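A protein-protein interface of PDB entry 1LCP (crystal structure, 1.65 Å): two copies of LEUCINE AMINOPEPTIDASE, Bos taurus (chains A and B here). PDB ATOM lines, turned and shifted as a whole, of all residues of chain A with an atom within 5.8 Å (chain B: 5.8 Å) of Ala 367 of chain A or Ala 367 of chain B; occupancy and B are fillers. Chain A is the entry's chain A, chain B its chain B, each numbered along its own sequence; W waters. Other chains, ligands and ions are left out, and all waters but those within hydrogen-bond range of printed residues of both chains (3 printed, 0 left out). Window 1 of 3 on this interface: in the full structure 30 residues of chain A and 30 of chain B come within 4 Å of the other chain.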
ATOM      1  N   GLY A 362      23.553  21.728 -18.749  1.00  0.00           N
ATOM      2  CA  GLY A 362      23.477  20.869 -19.919  1.00  0.00           C
ATOM      3  C   GLY A 362      23.744  21.745 -21.138  1.00  0.00           C
ATOM      4  O   GLY A 362      24.269  21.284 -22.157  1.00  0.00           O
ATOM      5  N   ALA A 363      23.401  23.030 -21.021  1.00  0.00           N
ATOM      6  CA  ALA A 363      23.608  23.999 -22.103  1.00  0.00           C
ATOM      7  C   ALA A 363      25.075  24.076 -22.542  1.00  0.00           C
ATOM      8  O   ALA A 363      25.361  24.207 -23.736  1.00  0.00           O
ATOM      9  CB  ALA A 363      23.107  25.376 -21.683  1.00  0.00           C
ATOM     10  N   MET A 364      25.997  23.971 -21.585  1.00  0.00           N
ATOM     11  CA  MET A 364      27.426  24.005 -21.904  1.00  0.00           C
ATOM     12  C   MET A 364      27.776  22.792 -22.776  1.00  0.00           C
ATOM     13  O   MET A 364      28.610  22.893 -23.689  1.00  0.00           O
ATOM     14  CB  MET A 364      28.262  23.997 -20.622  1.00  0.00           C
ATOM     15  CG  MET A 364      29.754  24.268 -20.838  1.00  0.00           C
ATOM     16  SD  MET A 364      30.127  25.956 -21.443  1.00  0.00           S
ATOM     17  CE  MET A 364      30.893  25.585 -22.893  1.00  0.00           C
ATOM     18  N   ASP A 365      27.148  21.646 -22.494  1.00  0.00           N
ATOM     19  CA  ASP A 365      27.397  20.450 -23.299  1.00  0.00           C
ATOM     20  C   ASP A 365      26.865  20.658 -24.735  1.00  0.00           C
ATOM     21  O   ASP A 365      27.504  20.274 -25.715  1.00  0.00           O
ATOM     22  CB  ASP A 365      26.749  19.220 -22.675  1.00  0.00           C
ATOM     23  CG  ASP A 365      27.039  17.963 -23.471  1.00  0.00           C
ATOM     24  OD1 ASP A 365      28.223  17.610 -23.625  1.00  0.00           O
ATOM     25  OD2 ASP A 365      26.090  17.358 -23.996  1.00  0.00           O
ATOM     26  N   ILE A 366      25.687  21.264 -24.851  1.00  0.00           N
ATOM     27  CA  ILE A 366      25.113  21.533 -26.165  1.00  0.00           C
ATOM     28  C   ILE A 366      26.007  22.542 -26.915  1.00  0.00           C
ATOM     29  O   ILE A 366      26.160  22.462 -28.138  1.00  0.00           O
ATOM     30  CB  ILE A 366      23.681  22.106 -26.053  1.00  0.00           C
ATOM     31  CG1 ILE A 366      22.742  21.039 -25.487  1.00  0.00           C
ATOM     32  CG2 ILE A 366      23.185  22.609 -27.421  1.00  0.00           C
ATOM     33  CD1 ILE A 366      22.717  19.763 -26.299  1.00  0.00           C
ATOM     34  N   ALA A 367      26.637  23.442 -26.164  1.00  0.00           N
ATOM     35  CA  ALA A 367      27.511  24.464 -26.738  1.00  0.00           C
ATOM     36  C   ALA A 367      28.854  23.978 -27.299  1.00  0.00           C
ATOM     37  O   ALA A 367      29.157  24.213 -28.479  1.00  0.00           O
ATOM     38  CB  ALA A 367      27.750  25.580 -25.727  1.00  0.00           C
ATOM     39  N   LEU A 368      29.653  23.318 -26.459  1.00  0.00           N
ATOM     40  CA  LEU A 368      30.994  22.865 -26.861  1.00  0.00           C
ATOM     41  C   LEU A 368      31.282  21.370 -26.705  1.00  0.00           C
ATOM     42  O   LEU A 368      32.354  20.891 -27.088  1.00  0.00           O
ATOM     43  CB  LEU A 368      32.054  23.662 -26.085  1.00  0.00           C
ATOM     44  CG  LEU A 368      32.014  25.197 -26.176  1.00  0.00           C
ATOM     45  CD1 LEU A 368      33.124  25.786 -25.318  1.00  0.00           C
ATOM     46  CD2 LEU A 368      32.155  25.666 -27.620  1.00  0.00           C
ATOM     47  N   GLY A 369      30.342  20.636 -26.127  1.00  0.00           N
ATOM     48  CA  GLY A 369      30.532  19.206 -25.940  1.00  0.00           C
ATOM     49  C   GLY A 369      31.772  18.928 -25.114  1.00  0.00           C
ATOM     50  O   GLY A 369      32.037  19.655 -24.153  1.00  0.00           O
ATOM     51  N   MET A 400      33.943  32.012 -22.758  1.00  0.00           N
ATOM     52  CA  MET A 400      32.505  32.257 -22.937  1.00  0.00           C
ATOM     53  C   MET A 400      32.224  33.658 -22.333  1.00  0.00           C
ATOM     54  O   MET A 400      32.854  34.046 -21.355  1.00  0.00           O
ATOM     55  CB  MET A 400      31.688  31.136 -22.287  1.00  0.00           C
ATOM     56  CG  MET A 400      31.880  29.761 -22.953  1.00  0.00           C
ATOM     57  SD  MET A 400      31.232  29.653 -24.669  1.00  0.00           S
ATOM     58  CE  MET A 400      29.483  29.442 -24.352  1.00  0.00           C
ATOM     59  N   TYR A 406      23.040  39.066 -20.242  1.00  0.00           N
ATOM     60  CA  TYR A 406      22.608  37.844 -19.567  1.00  0.00           C
ATOM     61  C   TYR A 406      22.140  38.117 -18.127  1.00  0.00           C
ATOM     62  O   TYR A 406      21.143  37.541 -17.671  1.00  0.00           O
ATOM     63  CB  TYR A 406      23.736  36.795 -19.617  1.00  0.00           C
ATOM     64  CG  TYR A 406      24.211  36.473 -21.038  1.00  0.00           C
ATOM     65  CD1 TYR A 406      23.359  35.855 -21.967  1.00  0.00           C
ATOM     66  CD2 TYR A 406      25.499  36.817 -21.461  1.00  0.00           C
ATOM     67  CE1 TYR A 406      23.777  35.595 -23.291  1.00  0.00           C
ATOM     68  CE2 TYR A 406      25.930  36.564 -22.772  1.00  0.00           C
ATOM     69  CZ  TYR A 406      25.064  35.957 -23.682  1.00  0.00           C
ATOM     70  OH  TYR A 406      25.482  35.734 -24.978  1.00  0.00           O
ATOM     71  N   ALA A 427      20.943  30.614 -24.305  1.00  0.00           N
ATOM     72  CA  ALA A 427      22.178  30.884 -23.547  1.00  0.00           C
ATOM     73  C   ALA A 427      22.220  30.400 -22.097  1.00  0.00           C
ATOM     74  O   ALA A 427      22.737  31.092 -21.225  1.00  0.00           O
ATOM     75  CB  ALA A 427      22.523  32.382 -23.636  1.00  0.00           C
ATOM     76  N   GLY A 428      21.732  29.184 -21.866  1.00  0.00           N
ATOM     77  CA  GLY A 428      21.703  28.623 -20.519  1.00  0.00           C
ATOM     78  C   GLY A 428      22.996  28.699 -19.722  1.00  0.00           C
ATOM     79  O   GLY A 428      22.962  28.996 -18.525  1.00  0.00           O
ATOM     80  N   ALA A 429      24.138  28.434 -20.354  1.00  0.00           N
ATOM     81  CA  ALA A 429      25.411  28.493 -19.632  1.00  0.00           C
ATOM     82  C   ALA A 429      25.796  29.931 -19.264  1.00  0.00           C
ATOM     83  O   ALA A 429      26.387  30.172 -18.207  1.00  0.00           O
ATOM     84  CB  ALA A 429      26.521  27.836 -20.459  1.00  0.00           C
ATOM     85  N   CYS A 430      25.421  30.875 -20.126  1.00  0.00           N
ATOM     86  CA  CYS A 430      25.719  32.297 -19.928  1.00  0.00           C
ATOM     87  C   CYS A 430      24.861  32.940 -18.830  1.00  0.00           C
ATOM     88  O   CYS A 430      25.359  33.751 -18.039  1.00  0.00           O
ATOM     89  CB  CYS A 430      25.578  33.066 -21.251  1.00  0.00           C
ATOM     90  SG  CYS A 430      26.661  32.469 -22.598  1.00  0.00           S
ATOM     91  N   GLY B 362      20.010  25.419 -33.907  1.00  0.00           N
ATOM     92  CA  GLY B 362      19.318  25.806 -32.692  1.00  0.00           C
ATOM     93  C   GLY B 362      20.335  25.743 -31.555  1.00  0.00           C
ATOM     94  O   GLY B 362      20.226  26.454 -30.555  1.00  0.00           O
ATOM     95  N   ALA B 363      21.358  24.906 -31.729  1.00  0.00           N
ATOM     96  CA  ALA B 363      22.409  24.748 -30.726  1.00  0.00           C
ATOM     97  C   ALA B 363      23.138  26.062 -30.463  1.00  0.00           C
ATOM     98  O   ALA B 363      23.520  26.343 -29.330  1.00  0.00           O
ATOM     99  CB  ALA B 363      23.404  23.668 -31.151  1.00  0.00           C
ATOM    100  N   MET B 364      23.303  26.886 -31.493  1.00  0.00           N
ATOM    101  CA  MET B 364      23.980  28.178 -31.335  1.00  0.00           C
ATOM    102  C   MET B 364      23.148  29.069 -30.405  1.00  0.00           C
ATOM    103  O   MET B 364      23.689  29.804 -29.574  1.00  0.00           O
ATOM    104  CB  MET B 364      24.160  28.859 -32.700  1.00  0.00           C
ATOM    105  CG  MET B 364      25.063  30.103 -32.686  1.00  0.00           C
ATOM    106  SD  MET B 364      26.831  29.757 -32.308  1.00  0.00           S
ATOM    107  CE  MET B 364      27.001  30.560 -30.788  1.00  0.00           C
ATOM    108  N   ASP B 365      21.826  28.975 -30.520  1.00  0.00           N
ATOM    109  CA  ASP B 365      20.933  29.764 -29.671  1.00  0.00           C
ATOM    110  C   ASP B 365      21.083  29.302 -28.210  1.00  0.00           C
ATOM    111  O   ASP B 365      21.147  30.119 -27.281  1.00  0.00           O
ATOM    112  CB  ASP B 365      19.482  29.616 -30.141  1.00  0.00           C
ATOM    113  CG  ASP B 365      18.537  30.484 -29.347  1.00  0.00           C
ATOM    114  OD1 ASP B 365      18.781  31.694 -29.295  1.00  0.00           O
ATOM    115  OD2 ASP B 365      17.594  29.954 -28.729  1.00  0.00           O
ATOM    116  N   ILE B 366      21.152  27.988 -28.017  1.00  0.00           N
ATOM    117  CA  ILE B 366      21.310  27.447 -26.682  1.00  0.00           C
ATOM    118  C   ILE B 366      22.676  27.874 -26.121  1.00  0.00           C
ATOM    119  O   ILE B 366      22.796  28.170 -24.925  1.00  0.00           O
ATOM    120  CB  ILE B 366      21.207  25.893 -26.690  1.00  0.00           C
ATOM    121  CG1 ILE B 366      19.793  25.453 -27.106  1.00  0.00           C
ATOM    122  CG2 ILE B 366      21.569  25.319 -25.318  1.00  0.00           C
ATOM    123  CD1 ILE B 366      18.683  25.949 -26.194  1.00  0.00           C
ATOM    124  N   ALA B 367      23.674  27.967 -26.999  1.00  0.00           N
ATOM    125  CA  ALA B 367      25.022  28.356 -26.591  1.00  0.00           C
ATOM    126  C   ALA B 367      25.184  29.829 -26.167  1.00  0.00           C
ATOM    127  O   ALA B 367      25.634  30.104 -25.049  1.00  0.00           O
ATOM    128  CB  ALA B 367      26.030  28.007 -27.697  1.00  0.00           C
ATOM    129  N   LEU B 368      24.821  30.766 -27.051  1.00  0.00           N
ATOM    130  CA  LEU B 368      24.981  32.200 -26.761  1.00  0.00           C
ATOM    131  C   LEU B 368      23.717  33.068 -26.861  1.00  0.00           C
ATOM    132  O   LEU B 368      23.752  34.254 -26.516  1.00  0.00           O
ATOM    133  CB  LEU B 368      26.074  32.799 -27.661  1.00  0.00           C
ATOM    134  CG  LEU B 368      27.482  32.174 -27.609  1.00  0.00           C
ATOM    135  CD1 LEU B 368      28.420  32.846 -28.607  1.00  0.00           C
ATOM    136  CD2 LEU B 368      28.052  32.298 -26.207  1.00  0.00           C
ATOM    137  N   GLY B 369      22.605  32.487 -27.302  1.00  0.00           N
ATOM    138  CA  GLY B 369      21.377  33.259 -27.435  1.00  0.00           C
ATOM    139  C   GLY B 369      21.554  34.457 -28.354  1.00  0.00           C
ATOM    140  O   GLY B 369      22.244  34.363 -29.373  1.00  0.00           O
ATOM    141  N   MET B 400      33.987  30.777 -31.686  1.00  0.00           N
ATOM    142  CA  MET B 400      33.626  29.387 -31.367  1.00  0.00           C
ATOM    143  C   MET B 400      34.716  28.488 -32.000  1.00  0.00           C
ATOM    144  O   MET B 400      35.251  28.816 -33.061  1.00  0.00           O
ATOM    145  CB  MET B 400      32.231  29.065 -31.892  1.00  0.00           C
ATOM    146  CG  MET B 400      31.111  29.840 -31.191  1.00  0.00           C
ATOM    147  SD  MET B 400      30.883  29.436 -29.425  1.00  0.00           S
ATOM    148  CE  MET B 400      29.899  27.921 -29.552  1.00  0.00           C
ATOM    149  N   TYR B 406      35.671  17.834 -33.579  1.00  0.00           N
ATOM    150  CA  TYR B 406      34.315  17.880 -34.126  1.00  0.00           C
ATOM    151  C   TYR B 406      34.223  17.258 -35.521  1.00  0.00           C
ATOM    152  O   TYR B 406      33.225  16.606 -35.852  1.00  0.00           O
ATOM    153  CB  TYR B 406      33.792  19.320 -34.115  1.00  0.00           C
ATOM    154  CG  TYR B 406      33.848  19.948 -32.736  1.00  0.00           C
ATOM    155  CD1 TYR B 406      33.065  19.461 -31.684  1.00  0.00           C
ATOM    156  CD2 TYR B 406      34.701  21.028 -32.476  1.00  0.00           C
ATOM    157  CE1 TYR B 406      33.135  20.036 -30.402  1.00  0.00           C
ATOM    158  CE2 TYR B 406      34.776  21.608 -31.203  1.00  0.00           C
ATOM    159  CZ  TYR B 406      33.993  21.109 -30.176  1.00  0.00           C
ATOM    160  OH  TYR B 406      34.081  21.686 -28.930  1.00  0.00           O
ATOM    161  N   ALA B 427      27.443  19.677 -28.733  1.00  0.00           N
ATOM    162  CA  ALA B 427      28.137  20.649 -29.570  1.00  0.00           C
ATOM    163  C   ALA B 427      27.623  20.787 -31.011  1.00  0.00           C
ATOM    164  O   ALA B 427      28.406  20.916 -31.955  1.00  0.00           O
ATOM    165  CB  ALA B 427      29.653  20.353 -29.553  1.00  0.00           C
ATOM    166  N   GLY B 428      26.306  20.818 -31.167  1.00  0.00           N
ATOM    167  CA  GLY B 428      25.707  20.930 -32.496  1.00  0.00           C
ATOM    168  C   GLY B 428      26.209  22.028 -33.427  1.00  0.00           C
ATOM    169  O   GLY B 428      26.305  21.818 -34.634  1.00  0.00           O
ATOM    170  N   ALA B 429      26.510  23.206 -32.887  1.00  0.00           N
ATOM    171  CA  ALA B 429      27.004  24.313 -33.711  1.00  0.00           C
ATOM    172  C   ALA B 429      28.428  24.019 -34.198  1.00  0.00           C
ATOM    173  O   ALA B 429      28.803  24.365 -35.329  1.00  0.00           O
ATOM    174  CB  ALA B 429      26.964  25.628 -32.924  1.00  0.00           C
ATOM    175  N   CYS B 430      29.205  23.360 -33.343  1.00  0.00           N
ATOM    176  CA  CYS B 430      30.584  23.001 -33.658  1.00  0.00           C
ATOM    177  C   CYS B 430      30.670  21.875 -34.704  1.00  0.00           C
ATOM    178  O   CYS B 430      31.532  21.915 -35.598  1.00  0.00           O
ATOM    179  CB  CYS B 430      31.326  22.628 -32.372  1.00  0.00           C
ATOM    180  SG  CYS B 430      31.390  23.951 -31.128  1.00  0.00           S
HETATM  181  O   HOH W   1      24.072  20.171 -29.675  1.00  0.00           O
HETATM  182  O   HOH W   2      24.837  28.348 -23.094  1.00  0.00           O
HETATM  183  O   HOH W   3      26.883  24.064 -30.219  1.00  0.00           O
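OH of Tyr 406 of chain A is in hydrogen-bond range of O of Leu 368 of chain B, 2.7 Å away. The backbone NH (N) of Ala 427 of chain A sits close to the backbone carbonyl oxygen (O) of Ile 366 of chain B (3.1 Å). The backbone carbonyl oxygen (O) of Asp 365 of chain A lies within hydrogen-bond range of the backbone NH (N) of Ala 427 of chain B. The side-chain sulfur of Cys 430 of chain A is in hydrogen-bond range of the backbone carbonyl oxygen of Ala 367 of chain B, at 3.6 Å. The backbone NH of Ala 427 of chain A is in hydrogen-bond range of the backbone carbonyl oxygen of Asp 365 of chain B. O of Ile 366 of chain A lies close to N of Ala 427 of chain B (3.1 Å). The side-chain hydroxyl of Tyr 406 of chain B sits at hydrogen-bond distance from the backbone carbonyl oxygen of Leu 368 of chain A (2.6 Å). O of Ala 367 of chain A lies within hydrogen-bond range of SG of Cys 430 of chain B, 3.5 Å away. The backbone carbonyl oxygen (O) of Ile 366 of chain A sits at hydrogen-bond distance from the backbone NH (N) of Gly 428 of chain B (3.4 Å). The backbone NH of Gly 428 of chain A sits at hydrogen-bond distance from the backbone carbonyl oxygen of Ile 366 of chain B (3.4 Å).
CG2 of Ile 366 of chain B touches CB of Ala 363 of chain A (3.9 Å). Ala 367 of chain A touches Ala 367 of chain B (CB to CB, 3.6 Å). Ala 367 of chain A touches Met 400 of chain B (O to CE, 3.9 Å). Leu 368 of chain A touches Met 400 of chain B. C of Leu 368 of chain A touches CB of Ala 427 of chain B, at 3.4 Å. Gly 369 of chain A touches Ala 427 of chain B (N to CB, 3.5 Å). Met 400 of chain A touches Ala 367 of chain B. Met 400 of chain A touches Leu 368 of chain B (CE to CD2, 3.7 Å). N of Gly 369 of chain B touches CB of Ala 427 of chain A, 3.7 Å away. Cys 430 of chain A touches Leu 368 of chain B.
Of the 14 printed residues of chain A, 11 touch a printed residue of chain B. Hydrophobic or aromatic side chains of chain A within 4 Å of the printed part of chain B: Ala 363, Ile 366, Ala 367, Leu 368, Met 400, Tyr 406 and Ala 427. Of the 14 printed residues of chain B, 11 touch a printed residue of chain A. Printed residues of chain B that touch a printed residue of chain A: Ala 363, Asp 365, Ile 366, Ala 367, Leu 368, Gly 369, Met 400, Tyr 406, Ala 427, Gly 428 and Cys 430. Among the printed residues, 26 pairs touch across the chains. Among the printed residues, no Asp or Glu carboxylate lies within 4 Å of a Lys or Arg side-chain nitrogen of the other chain.
Ala 367 of chain A touches four residues of chain B. Printed residues of chain A within 4 Å of Ala 367 of chain B: Ala 367 (3.6 Å), Met 400 (3.97 Å), Ala 427 (3.8 Å) and Cys 430 (3.6 Å). Printed residues of chain A within 4 Å of Leu 368 of chain B: Met 400 (3.7 Å), Tyr 406 (2.7 Å), Ala 427 (3.5 Å) and Cys 430 (3.9 Å). Printed residues of chain A within 4 Å of Gly 369 of chain B: Ala 427 (3.7 Å). The nearest printed residue of chain B that does not touch Cys 430 of chain A is Ile 366 of chain B (6.1 Å).
Water W3 lies within hydrogen-bond range of the backbone carbonyl oxygen of Ile 366 of chain A, the backbone NH of Ala 429 of chain B, the backbone carbonyl oxygen of Ala 367 of chain A and the backbone NH of Gly 428 of chain B. Water W2 lies within hydrogen-bond range of O of Ala 367 of chain B (2.7 Å), O of Ile 366 of chain B (2.7 Å), N of Ala 429 of chain A (2.8 Å) and N of Gly 428 of chain A (3.4 Å). Water W1 lies within hydrogen-bond range of the backbone NH of Gly 428 of chain B (2.8 Å) and the backbone carbonyl oxygen of Ile 366 of chain A (3.5 Å).
Ile 366 of chain A touches Gly 428 of chain B, and with the chains exchanged Gly 428 of chain A touches Ile 366 of chain B. Ala 367 of chain A touches Ala 427 of chain B, and with the chains exchanged Ala 427 of chain A touches Ala 367 of chain B. Leu 368 of chain A touches Tyr 406 of chain B, and with the chains exchanged Tyr 406 of chain A touches Leu 368 of chain B. Leu 368 of chain A touches Ala 427 of chain B, and with the chains exchanged Ala 427 of chain A touches Leu 368 of chain B. Of the 26 pairs that touch across the chains among the printed residues, 26 have their exchanged pair printed and touching as well.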
